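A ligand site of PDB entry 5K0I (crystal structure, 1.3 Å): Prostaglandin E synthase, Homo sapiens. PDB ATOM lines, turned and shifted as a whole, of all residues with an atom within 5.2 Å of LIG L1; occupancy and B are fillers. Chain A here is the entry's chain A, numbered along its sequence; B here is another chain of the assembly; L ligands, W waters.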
ATOM      1  N   ARG A  72       4.966   7.564  12.834  1.00  0.00           N
ATOM      2  CA  ARG A  72       6.177   8.288  13.241  1.00  0.00           C
ATOM      3  C   ARG A  72       7.092   8.567  12.066  1.00  0.00           C
ATOM      4  O   ARG A  72       7.637   9.675  11.962  1.00  0.00           O
ATOM      5  CB  ARG A  72       6.959   7.510  14.314  1.00  0.00           C
ATOM      6  CG  ARG A  72       6.269   7.461  15.668  1.00  0.00           C
ATOM      7  CD  ARG A  72       7.211   7.050  16.803  1.00  0.00           C
ATOM      8  NE  ARG A  72       7.684   5.668  16.710  1.00  0.00           N
ATOM      9  CZ  ARG A  72       6.986   4.606  17.102  1.00  0.00           C
ATOM     10  NH1 ARG A  72       5.767   4.753  17.587  1.00  0.00           N
ATOM     11  NH2 ARG A  72       7.520   3.387  16.994  1.00  0.00           N
ATOM     12  N   ARG A  75       5.424  11.312  10.064  1.00  0.00           N
ATOM     13  CA  ARG A  75       5.570  12.581  10.758  1.00  0.00           C
ATOM     14  C   ARG A  75       6.996  13.121  10.634  1.00  0.00           C
ATOM     15  O   ARG A  75       7.203  14.312  10.360  1.00  0.00           O
ATOM     16  CB  ARG A  75       5.163  12.462  12.221  1.00  0.00           C
ATOM     17  CG  ARG A  75       5.191  13.788  12.917  1.00  0.00           C
ATOM     18  CD  ARG A  75       4.794  13.696  14.365  1.00  0.00           C
ATOM     19  NE  ARG A  75       5.195  14.942  14.988  1.00  0.00           N
ATOM     20  CZ  ARG A  75       4.539  15.566  15.956  1.00  0.00           C
ATOM     21  NH1 ARG A  75       5.040  16.698  16.378  1.00  0.00           N
ATOM     22  NH2 ARG A  75       3.402  15.096  16.485  1.00  0.00           N
ATOM     23  N   ASN A  76       7.998  12.254  10.797  1.00  0.00           N
ATOM     24  CA  ASN A  76       9.374  12.689  10.669  1.00  0.00           C
ATOM     25  C   ASN A  76       9.652  13.224   9.257  1.00  0.00           C
ATOM     26  O   ASN A  76      10.346  14.228   9.104  1.00  0.00           O
ATOM     27  CB  ASN A  76      10.331  11.576  11.088  1.00  0.00           C
ATOM     28  CG  ASN A  76      11.749  12.064  11.242  1.00  0.00           C
ATOM     29  OD1 ASN A  76      12.480  12.204  10.262  1.00  0.00           O
ATOM     30  ND2 ASN A  76      12.144  12.366  12.476  1.00  0.00           N
ATOM     31  N   GLU A  79       8.401  16.673   9.130  1.00  0.00           N
ATOM     32  CA  GLU A  79       9.305  17.554   9.879  1.00  0.00           C
ATOM     33  C   GLU A  79      10.567  17.937   9.075  1.00  0.00           C
ATOM     34  O   GLU A  79      11.255  18.907   9.431  1.00  0.00           O
ATOM     35  CB  GLU A  79       9.705  16.886  11.208  1.00  0.00           C
ATOM     36  CG  GLU A  79       8.525  16.748  12.178  1.00  0.00           C
ATOM     37  CD  GLU A  79       8.821  15.898  13.405  1.00  0.00           C
ATOM     38  OE1 GLU A  79       9.962  15.394  13.570  1.00  0.00           O
ATOM     39  OE2 GLU A  79       7.885  15.702  14.211  1.00  0.00           O
ATOM     40  N   HIS A 115      16.539   6.688   5.854  1.00  0.00           N
ATOM     41  CA  HIS A 115      15.802   6.920   7.100  1.00  0.00           C
ATOM     42  C   HIS A 115      14.519   6.093   7.156  1.00  0.00           C
ATOM     43  O   HIS A 115      14.233   5.429   8.153  1.00  0.00           O
ATOM     44  CB  HIS A 115      15.493   8.403   7.284  1.00  0.00           C
ATOM     45  CG  HIS A 115      14.856   8.718   8.610  1.00  0.00           C
ATOM     46  ND1 HIS A 115      13.485   8.705   8.800  1.00  0.00           N
ATOM     47  CD2 HIS A 115      15.405   9.071   9.792  1.00  0.00           C
ATOM     48  CE1 HIS A 115      13.230   9.027  10.058  1.00  0.00           C
ATOM     49  NE2 HIS A 115      14.370   9.257  10.686  1.00  0.00           N
ATOM     50  N   TYR A 119      13.728   3.100   9.679  1.00  0.00           N
ATOM     51  CA  TYR A 119      12.600   3.256  10.597  1.00  0.00           C
ATOM     52  C   TYR A 119      11.626   2.084  10.459  1.00  0.00           C
ATOM     53  O   TYR A 119      11.348   1.383  11.432  1.00  0.00           O
ATOM     54  CB  TYR A 119      11.854   4.584  10.367  1.00  0.00           C
ATOM     55  CG  TYR A 119      11.345   5.207  11.653  1.00  0.00           C
ATOM     56  CD1 TYR A 119      11.190   4.453  12.808  1.00  0.00           C
ATOM     57  CD2 TYR A 119      11.036   6.570  11.711  1.00  0.00           C
ATOM     58  CE1 TYR A 119      10.759   5.017  14.001  1.00  0.00           C
ATOM     59  CE2 TYR A 119      10.604   7.159  12.908  1.00  0.00           C
ATOM     60  CZ  TYR A 119      10.464   6.372  14.045  1.00  0.00           C
ATOM     61  OH  TYR A 119      10.088   6.902  15.258  1.00  0.00           O
ATOM     62  N   ARG A 128      19.133   4.688  12.182  1.00  0.00           N
ATOM     63  CA  ARG A 128      18.135   5.707  11.811  1.00  0.00           C
ATOM     64  C   ARG A 128      18.608   7.118  12.194  1.00  0.00           C
ATOM     65  O   ARG A 128      18.514   8.055  11.393  1.00  0.00           O
ATOM     66  CB  ARG A 128      16.790   5.407  12.468  1.00  0.00           C
ATOM     67  CG  ARG A 128      15.641   6.283  11.942  1.00  0.00           C
ATOM     68  CD  ARG A 128      14.446   6.259  12.874  1.00  0.00           C
ATOM     69  NE  ARG A 128      14.689   6.980  14.114  1.00  0.00           N
ATOM     70  CZ  ARG A 128      14.919   6.431  15.305  1.00  0.00           C
ATOM     71  NH1 ARG A 128      14.942   5.105  15.470  1.00  0.00           N
ATOM     72  NH2 ARG A 128      15.133   7.216  16.351  1.00  0.00           N
ATOM     73  N   SER A 129      19.119   7.275  13.414  1.00  0.00           N
ATOM     74  CA  SER A 129      19.594   8.579  13.887  1.00  0.00           C
ATOM     75  C   SER A 129      20.724   9.145  13.017  1.00  0.00           C
ATOM     76  O   SER A 129      20.766  10.361  12.756  1.00  0.00           O
ATOM     77  CB  SER A 129      20.037   8.504  15.351  1.00  0.00           C
ATOM     78  OG  SER A 129      18.959   8.106  16.181  1.00  0.00           O
ATOM     79  N   TYR A 132      19.236  10.323   9.666  1.00  0.00           N
ATOM     80  CA  TYR A 132      18.548  11.589   9.909  1.00  0.00           C
ATOM     81  C   TYR A 132      19.551  12.741   9.904  1.00  0.00           C
ATOM     82  O   TYR A 132      19.344  13.769   9.244  1.00  0.00           O
ATOM     83  CB  TYR A 132      17.801  11.549  11.263  1.00  0.00           C
ATOM     84  CG  TYR A 132      17.060  12.828  11.536  1.00  0.00           C
ATOM     85  CD1 TYR A 132      17.700  13.926  12.122  1.00  0.00           C
ATOM     86  CD2 TYR A 132      15.721  12.969  11.171  1.00  0.00           C
ATOM     87  CE1 TYR A 132      17.010  15.122  12.340  1.00  0.00           C
ATOM     88  CE2 TYR A 132      15.030  14.154  11.380  1.00  0.00           C
ATOM     89  CZ  TYR A 132      15.678  15.232  11.967  1.00  0.00           C
ATOM     90  OH  TYR A 132      15.003  16.400  12.182  1.00  0.00           O
ATOM     91  N   ALA B  33      13.250  20.436  16.908  1.00  0.00           N
ATOM     92  CA  ALA B  33      13.622  19.033  16.689  1.00  0.00           C
ATOM     93  C   ALA B  33      14.814  18.614  17.559  1.00  0.00           C
ATOM     94  O   ALA B  33      14.811  17.545  18.156  1.00  0.00           O
ATOM     95  CB  ALA B  33      13.925  18.768  15.208  1.00  0.00           C
ATOM     96  N   THR B  36      13.807  18.437  21.204  1.00  0.00           N
ATOM     97  CA  THR B  36      13.050  17.207  21.417  1.00  0.00           C
ATOM     98  C   THR B  36      13.982  16.020  21.659  1.00  0.00           C
ATOM     99  O   THR B  36      13.788  15.262  22.606  1.00  0.00           O
ATOM    100  CB  THR B  36      12.114  16.895  20.223  1.00  0.00           C
ATOM    101  OG1 THR B  36      11.260  18.018  19.988  1.00  0.00           O
ATOM    102  CG2 THR B  36      11.254  15.667  20.491  1.00  0.00           C
ATOM    103  N   GLY B  37      14.994  15.886  20.819  1.00  0.00           N
ATOM    104  CA  GLY B  37      15.998  14.833  20.977  1.00  0.00           C
ATOM    105  C   GLY B  37      16.718  14.898  22.316  1.00  0.00           C
ATOM    106  O   GLY B  37      16.910  13.863  22.965  1.00  0.00           O
ATOM    107  N   ARG B  40      14.348  13.697  25.031  1.00  0.00           N
ATOM    108  CA  ARG B  40      14.272  12.229  24.983  1.00  0.00           C
ATOM    109  C   ARG B  40      15.459  11.574  25.681  1.00  0.00           C
ATOM    110  O   ARG B  40      15.284  10.639  26.457  1.00  0.00           O
ATOM    111  CB  ARG B  40      14.209  11.733  23.531  1.00  0.00           C
ATOM    112  CG  ARG B  40      12.887  12.029  22.824  1.00  0.00           C
ATOM    113  CD  ARG B  40      12.810  11.237  21.524  1.00  0.00           C
ATOM    114  NE  ARG B  40      11.558  11.407  20.800  1.00  0.00           N
ATOM    115  CZ  ARG B  40      10.411  10.789  21.103  1.00  0.00           C
ATOM    116  NH1 ARG B  40      10.315   9.998  22.176  1.00  0.00           N
ATOM    117  NH2 ARG B  40       9.325  10.981  20.350  1.00  0.00           N
ATOM    118  N   ALA B  47      10.900   6.674  21.592  1.00  0.00           N
ATOM    119  CA  ALA B  47       9.694   6.237  20.920  1.00  0.00           C
ATOM    120  C   ALA B  47       9.783   4.824  20.380  1.00  0.00           C
ATOM    121  O   ALA B  47       8.771   4.224  20.014  1.00  0.00           O
ATOM    122  CB  ALA B  47       9.369   7.187  19.781  1.00  0.00           C
ATOM    123  N   ASN B  48      11.009   4.283  20.330  1.00  0.00           N
ATOM    124  CA  ASN B  48      11.267   3.011  19.655  1.00  0.00           C
ATOM    125  C   ASN B  48      12.066   2.064  20.535  1.00  0.00           C
ATOM    126  O   ASN B  48      13.018   2.511  21.193  1.00  0.00           O
ATOM    127  CB  ASN B  48      12.039   3.275  18.356  1.00  0.00           C
ATOM    128  CG  ASN B  48      11.325   4.253  17.464  1.00  0.00           C
ATOM    129  OD1 ASN B  48      10.255   3.957  16.952  1.00  0.00           O
ATOM    130  ND2 ASN B  48      11.925   5.440  17.282  1.00  0.00           N
ATOM    131  N   LEU B  71       6.707  17.736  21.013  1.00  0.00           N
ATOM    132  CA  LEU B  71       6.033  17.268  19.809  1.00  0.00           C
ATOM    133  C   LEU B  71       4.820  18.136  19.460  1.00  0.00           C
ATOM    134  O   LEU B  71       4.580  18.388  18.282  1.00  0.00           O
ATOM    135  CB  LEU B  71       5.647  15.799  19.912  1.00  0.00           C
ATOM    136  CG  LEU B  71       6.800  14.795  19.835  1.00  0.00           C
ATOM    137  CD1 LEU B  71       6.323  13.445  20.351  1.00  0.00           C
ATOM    138  CD2 LEU B  71       7.331  14.687  18.404  1.00  0.00           C
ATOM    139  N   HIS B  74       6.141  21.334  17.904  1.00  0.00           N
ATOM    140  CA  HIS B  74       6.604  21.044  16.548  1.00  0.00           C
ATOM    141  C   HIS B  74       5.425  20.834  15.601  1.00  0.00           C
ATOM    142  O   HIS B  74       5.421  21.338  14.454  1.00  0.00           O
ATOM    143  CB  HIS B  74       7.520  19.824  16.569  1.00  0.00           C
ATOM    144  CG  HIS B  74       8.490  19.762  15.435  1.00  0.00           C
ATOM    145  ND1 HIS B  74       9.549  18.882  15.429  1.00  0.00           N
ATOM    146  CD2 HIS B  74       8.555  20.452  14.267  1.00  0.00           C
ATOM    147  CE1 HIS B  74      10.238  19.040  14.307  1.00  0.00           C
ATOM    148  NE2 HIS B  74       9.663  19.997  13.586  1.00  0.00           N
HETATM  149  N1  LIG L   1      10.144  14.654  16.319  1.00  0.00           N
HETATM  150  C1  LIG L   1      11.455  14.022  16.437  1.00  0.00           C
HETATM  151  C2  LIG L   1      11.469  13.002  17.548  1.00  0.00           C
HETATM  152  O1  LIG L   1      12.444  12.223  17.650  1.00  0.00           O
HETATM  153  O2  LIG L   1      10.500  12.924  18.338  1.00  0.00           O
HETATM  154  C3  LIG L   1      12.529  15.115  16.655  1.00  0.00           C
HETATM  155  C4  LIG L   1      13.979  14.612  16.670  1.00  0.00           C
HETATM  156  C5  LIG L   1      14.280  13.723  15.493  1.00  0.00           C
HETATM  157  O3  LIG L   1      13.766  14.009  14.272  1.00  0.00           O
HETATM  158  N2  LIG L   1      15.040  12.652  15.657  1.00  0.00           N
HETATM  159  C6  LIG L   1      15.311  11.706  14.583  1.00  0.00           C
HETATM  160  C7  LIG L   1      14.226  10.672  14.454  1.00  0.00           C
HETATM  161  O4  LIG L   1      14.357   9.729  13.488  1.00  0.00           O
HETATM  162  C8  LIG L   1      16.657  11.029  14.833  1.00  0.00           C
HETATM  163  S1  LIG L   1      16.716  10.207  16.447  1.00  0.00           S
HETATM  164  N3  LIG L   1      13.194  10.674  15.282  1.00  0.00           N
HETATM  165  C9  LIG L   1      12.156   9.665  15.238  1.00  0.00           C
HETATM  166  C10 LIG L   1      10.767  10.234  15.125  1.00  0.00           C
HETATM  167  O5  LIG L   1      10.605  11.449  14.783  1.00  0.00           O
HETATM  168  O6  LIG L   1       9.779   9.480  15.347  1.00  0.00           O
HETATM  169  O1  LG2 L   2      18.632   8.666  20.089  1.00  0.00           O
HETATM  170  C1  LG2 L   2      18.982  20.411  11.730  1.00  0.00           C
HETATM  171  O2  LG2 L   2      21.428   8.664  20.909  1.00  0.00           O
HETATM  172  C2  LG2 L   2      20.321  20.465  11.366  1.00  0.00           C
HETATM  173  C3  LG2 L   2      19.383  18.433  13.036  1.00  0.00           C
HETATM  174  N1  LG2 L   2      19.162  15.563  15.112  1.00  0.00           N
HETATM  175  C4  LG2 L   2      21.188  19.515  11.807  1.00  0.00           C
HETATM  176  C5  LG2 L   2      21.095  16.481  13.962  1.00  0.00           C
HETATM  177  C6  LG2 L   2      21.591  17.456  13.145  1.00  0.00           C
HETATM  178  C7  LG2 L   2      20.753  18.479  12.652  1.00  0.00           C
HETATM  179  O3  LG2 L   2      18.912  14.119  19.675  1.00  0.00           O
HETATM  180  C8  LG2 L   2      18.478  13.398  18.791  1.00  0.00           C
HETATM  181  N2  LG2 L   2      18.004  12.162  19.032  1.00  0.00           N
HETATM  182  C9  LG2 L   2      18.194  11.493  20.327  1.00  0.00           C
HETATM  183  C10 LG2 L   2      17.080  10.472  20.594  1.00  0.00           C
HETATM  184  C11 LG2 L   2      17.290   9.148  19.892  1.00  0.00           C
HETATM  185  C12 LG2 L   2      19.604   9.558  19.566  1.00  0.00           C
HETATM  186  C13 LG2 L   2      20.928   8.843  19.590  1.00  0.00           C
HETATM  187  C14 LG2 L   2      19.570  10.828  20.392  1.00  0.00           C
HETATM  188  C15 LG2 L   2      18.438  13.835  17.342  1.00  0.00           C
HETATM  189  C16 LG2 L   2      19.819  13.684  16.641  1.00  0.00           C
HETATM  190  C17 LG2 L   2      20.952  14.476  17.327  1.00  0.00           C
HETATM  191  C18 LG2 L   2      20.270  12.217  16.581  1.00  0.00           C
HETATM  192  C19 LG2 L   2      19.687  14.195  15.200  1.00  0.00           C
HETATM  193  C20 LG2 L   2      17.864  15.268  17.207  1.00  0.00           C
HETATM  194  C21 LG2 L   2      17.845  15.719  15.736  1.00  0.00           C
HETATM  195  C22 LG2 L   2      19.727  16.514  14.289  1.00  0.00           C
HETATM  196  C23 LG2 L   2      18.484  19.431  12.554  1.00  0.00           C
HETATM  197  C24 LG2 L   2      17.025  19.390  12.950  1.00  0.00           C
HETATM  198  N3  LG2 L   2      18.898  17.448  13.862  1.00  0.00           N
HETATM  199  O   HOH W   1       9.882  17.123  17.560  1.00  0.00           O
HETATM  200  O   HOH W   2      13.975  10.090  18.512  1.00  0.00           O
HETATM  201  O   HOH W   3      11.167   9.461  18.321  1.00  0.00           O
HETATM  202  O   HOH W   4      12.495  16.101  13.059  1.00  0.00           O
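OH of Tyr 119 sits at hydrogen-bond distance from NE of Arg 72 (3.1 Å). OH of Tyr 119 sits at hydrogen-bond distance from ND2 of Asn 48 of chain B. The side-chain carboxylate of Glu 79 is in salt-bridge range of the guanidinium group of Arg 75. O of Leu 71 of chain B is in hydrogen-bond range of NH1 of Arg 75, 2.6 Å away. NH2 of Arg 72 is in hydrogen-bond range of OD1 of Asn 48 of chain B (2.8 Å). The backbone carbonyl oxygen (O) of Ala 47 of chain B sits at hydrogen-bond distance from the guanidinium group (NH2) of Arg 72, at 3.4 Å.
The side-chain hydroxyl (OH) of Tyr 119 is in hydrogen-bond range of an oxygen (O6) of LIG L1. An oxygen (O4) of LIG L1 lies within hydrogen-bond range of the guanidinium group (NE) of Arg 128. NE2 of His 115 sits at hydrogen-bond distance from O4 of LIG L1 (2.8 Å). OE1 of Glu 79 lies within salt-bridge range of N1 of LIG L1, at 2.9 Å. The side-chain amide nitrogen (ND2) of Asn 76 is in hydrogen-bond range of an oxygen (O5) of LIG L1. O2 of LIG L1 lies within salt-bridge range of NH2 of Arg 40 of chain B, at 3.0 Å. The side-chain hydroxyl (OG) of Ser 129 sits close to a sulfur (S1) of LIG L1. An oxygen (O3) of LIG L1 lies close to the side-chain hydroxyl (OH) of Tyr 132, 3.4 Å away.
A sulfur (S1) of LIG L1 sits close to a nitrogen (N2) of LG2 L2, at 3.5 Å.
Water W4 lies within hydrogen-bond range of the side-chain hydroxyl of Tyr 132 (2.7 Å), the side-chain carboxylate of Glu 79 (2.7 Å) and an oxygen (O3) of LIG L1 (2.7 Å). Water W1 lies within hydrogen-bond range of a nitrogen (N1) of LIG L1 (2.8 Å), a ring nitrogen (ND1) of His 74 of chain B (2.8 Å) and the side-chain hydroxyl (OG1) of Thr 36 of chain B (2.9 Å). Water W3 bridges an oxygen (O1) of LIG L1 (3.1 Å) and the guanidinium group (NH2) of Arg 40 of chain B (3.1 Å).
CB of Arg 72 touches O6 of LIG L1, at 3.6 Å. O of Ala 33 of chain B touches C4 of LIG L1 (3.4 Å). Thr 36 of chain B touches LIG L1. Leu 71 of chain B touches LIG L1 (CD2 to N1, 3.5 Å). Within 4 Å of LIG L1: Arg 72, Asn 76, Glu 79, His 115, Tyr 119, Arg 128, Ser 129, Tyr 132, Ala 33 of chain B, Thr 36 of chain B, Arg 40 of chain B and Leu 71 of chain B.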
